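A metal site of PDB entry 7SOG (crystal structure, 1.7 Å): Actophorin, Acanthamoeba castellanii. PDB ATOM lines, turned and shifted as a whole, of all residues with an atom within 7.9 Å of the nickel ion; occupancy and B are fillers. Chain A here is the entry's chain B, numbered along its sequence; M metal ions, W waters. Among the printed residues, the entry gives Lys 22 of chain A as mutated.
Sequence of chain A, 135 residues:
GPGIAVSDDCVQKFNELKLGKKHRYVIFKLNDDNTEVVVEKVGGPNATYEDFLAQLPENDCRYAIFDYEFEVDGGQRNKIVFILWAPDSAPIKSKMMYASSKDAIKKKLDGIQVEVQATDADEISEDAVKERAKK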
ATOM      1  N   GLN A  12       3.326 -10.298  16.314  1.00  0.00           N
ATOM      2  CA  GLN A  12       4.079  -9.608  15.279  1.00  0.00           C
ATOM      3  C   GLN A  12       3.614  -8.170  15.128  1.00  0.00           C
ATOM      4  O   GLN A  12       4.427  -7.240  15.053  1.00  0.00           O
ATOM      5  CB  GLN A  12       3.935 -10.342  13.934  1.00  0.00           C
ATOM      6  CG  GLN A  12       4.901  -9.854  12.863  1.00  0.00           C
ATOM      7  CD  GLN A  12       4.481 -10.252  11.463  1.00  0.00           C
ATOM      8  OE1 GLN A  12       4.464  -9.423  10.542  1.00  0.00           O
ATOM      9  NE2 GLN A  12       4.149 -11.528  11.292  1.00  0.00           N
ATOM     10  N   LYS A  13       2.298  -7.950  15.074  1.00  0.00           N
ATOM     11  CA  LYS A  13       1.786  -6.593  14.899  1.00  0.00           C
ATOM     12  C   LYS A  13       2.075  -5.734  16.118  1.00  0.00           C
ATOM     13  O   LYS A  13       2.384  -4.559  15.971  1.00  0.00           O
ATOM     14  CB  LYS A  13       0.284  -6.638  14.611  1.00  0.00           C
ATOM     15  CG  LYS A  13      -0.023  -6.998  13.183  1.00  0.00           C
ATOM     16  CD  LYS A  13       0.367  -5.836  12.284  1.00  0.00           C
ATOM     17  CE  LYS A  13       1.344  -6.240  11.213  1.00  0.00           C
ATOM     18  NZ  LYS A  13       1.115  -5.484   9.945  1.00  0.00           N
ATOM     19  N   GLU A  16       5.609  -4.536  15.937  1.00  0.00           N
ATOM     20  CA  GLU A  16       5.735  -3.426  15.001  1.00  0.00           C
ATOM     21  C   GLU A  16       5.266  -2.126  15.635  1.00  0.00           C
ATOM     22  O   GLU A  16       5.907  -1.078  15.518  1.00  0.00           O
ATOM     23  CB  GLU A  16       4.948  -3.713  13.728  1.00  0.00           C
ATOM     24  CG  GLU A  16       5.534  -4.799  12.860  1.00  0.00           C
ATOM     25  CD  GLU A  16       4.809  -4.979  11.551  1.00  0.00           C
ATOM     26  OE1 GLU A  16       3.843  -4.231  11.303  1.00  0.00           O
ATOM     27  OE2 GLU A  16       5.195  -5.868  10.752  1.00  0.00           O
ATOM     28  N   LEU A  17       4.110  -2.161  16.305  1.00  0.00           N
ATOM     29  CA  LEU A  17       3.637  -0.986  17.030  1.00  0.00           C
ATOM     30  C   LEU A  17       4.679  -0.527  18.035  1.00  0.00           C
ATOM     31  O   LEU A  17       4.972   0.663  18.142  1.00  0.00           O
ATOM     32  CB  LEU A  17       2.306  -1.309  17.712  1.00  0.00           C
ATOM     33  CG  LEU A  17       1.644  -0.253  18.594  1.00  0.00           C
ATOM     34  CD1 LEU A  17       0.125  -0.428  18.507  1.00  0.00           C
ATOM     35  CD2 LEU A  17       2.094  -0.348  20.033  1.00  0.00           C
ATOM     36  N   LYS A  22       5.045   2.425  12.459  1.00  0.00           N
ATOM     37  CA  LYS A  22       4.467   1.356  11.658  1.00  0.00           C
ATOM     38  C   LYS A  22       2.959   1.245  11.812  1.00  0.00           C
ATOM     39  O   LYS A  22       2.229   1.231  10.813  1.00  0.00           O
ATOM     40  CB  LYS A  22       5.133   0.019  12.025  1.00  0.00           C
ATOM     41  CG  LYS A  22       6.217  -0.445  11.062  1.00  0.00           C
ATOM     42  CD  LYS A  22       5.691  -0.647   9.629  1.00  0.00           C
ATOM     43  CE  LYS A  22       4.498  -1.607   9.543  1.00  0.00           C
ATOM     44  NZ  LYS A  22       3.614  -1.310   8.363  1.00  0.00           N
ATOM     45  N   HIS A  23       2.455   1.186  13.046  1.00  0.00           N
ATOM     46  CA  HIS A  23       1.022   1.052  13.272  1.00  0.00           C
ATOM     47  C   HIS A  23       0.644   1.833  14.526  1.00  0.00           C
ATOM     48  O   HIS A  23       1.243   1.610  15.594  1.00  0.00           O
ATOM     49  CB  HIS A  23       0.635  -0.428  13.419  1.00  0.00           C
ATOM     50  CG  HIS A  23       0.871  -1.231  12.180  1.00  0.00           C
ATOM     51  ND1 HIS A  23       0.206  -0.983  11.006  1.00  0.00           N
ATOM     52  CD2 HIS A  23       1.699  -2.265  11.928  1.00  0.00           C
ATOM     53  CE1 HIS A  23       0.616  -1.843  10.084  1.00  0.00           C
ATOM     54  NE2 HIS A  23       1.524  -2.630  10.618  1.00  0.00           N
ATOM     55  N   VAL A  26      -3.757  -1.522  17.062  1.00  0.00           N
ATOM     56  CA  VAL A  26      -4.175  -2.831  16.585  1.00  0.00           C
ATOM     57  C   VAL A  26      -5.383  -3.241  17.400  1.00  0.00           C
ATOM     58  O   VAL A  26      -5.417  -2.988  18.611  1.00  0.00           O
ATOM     59  CB  VAL A  26      -3.060  -3.893  16.706  1.00  0.00           C
ATOM     60  CG1 VAL A  26      -3.560  -5.239  16.163  1.00  0.00           C
ATOM     61  CG2 VAL A  26      -1.821  -3.436  15.967  1.00  0.00           C
ATOM     62  N   VAL A  42      -5.887  -3.314  11.832  1.00  0.00           N
ATOM     63  CA  VAL A  42      -4.614  -2.636  12.063  1.00  0.00           C
ATOM     64  C   VAL A  42      -4.772  -1.196  11.627  1.00  0.00           C
ATOM     65  O   VAL A  42      -5.355  -0.919  10.573  1.00  0.00           O
ATOM     66  CB  VAL A  42      -3.467  -3.315  11.292  1.00  0.00           C
ATOM     67  CG1 VAL A  42      -2.152  -2.645  11.660  1.00  0.00           C
ATOM     68  CG2 VAL A  42      -3.429  -4.806  11.610  1.00  0.00           C
ATOM     69  N   GLY A  43      -4.297  -0.271  12.451  1.00  0.00           N
ATOM     70  CA  GLY A  43      -4.306   1.126  12.099  1.00  0.00           C
ATOM     71  C   GLY A  43      -3.003   1.516  11.408  1.00  0.00           C
ATOM     72  O   GLY A  43      -1.945   1.023  11.752  1.00  0.00           O
HETATM   73 NI    NI M   1       2.676  -4.083   9.692  1.00  0.00          NI
HETATM   74  O   HOH W   1       4.000  -5.299   8.661  1.00  0.00           O
HETATM   75  O   HOH W   2       1.526  -3.891   8.209  1.00  0.00           O
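The side-chain amino group (NZ) of Lys 22 sits close to a ring nitrogen (NE2) of His 23, at 3.3 Å. O of Gly 43 is in hydrogen-bond range of ND1 of His 23 (3.0 Å).
Lys 22 touches the nickel ion. Of the 9 residues printed, 4 come within 4 Å of the nickel ion.
Water W2 is bound to the nickel ion (1.9 Å). OE1 of Glu 16 is bound to the nickel ion (2.0 Å). The nickel ion is bound by water W1 (2.1 Å). NE2 of His 23 binds the nickel ion, 2.1 Å away. NZ of Lys 13 binds the nickel ion, at 2.1 Å.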
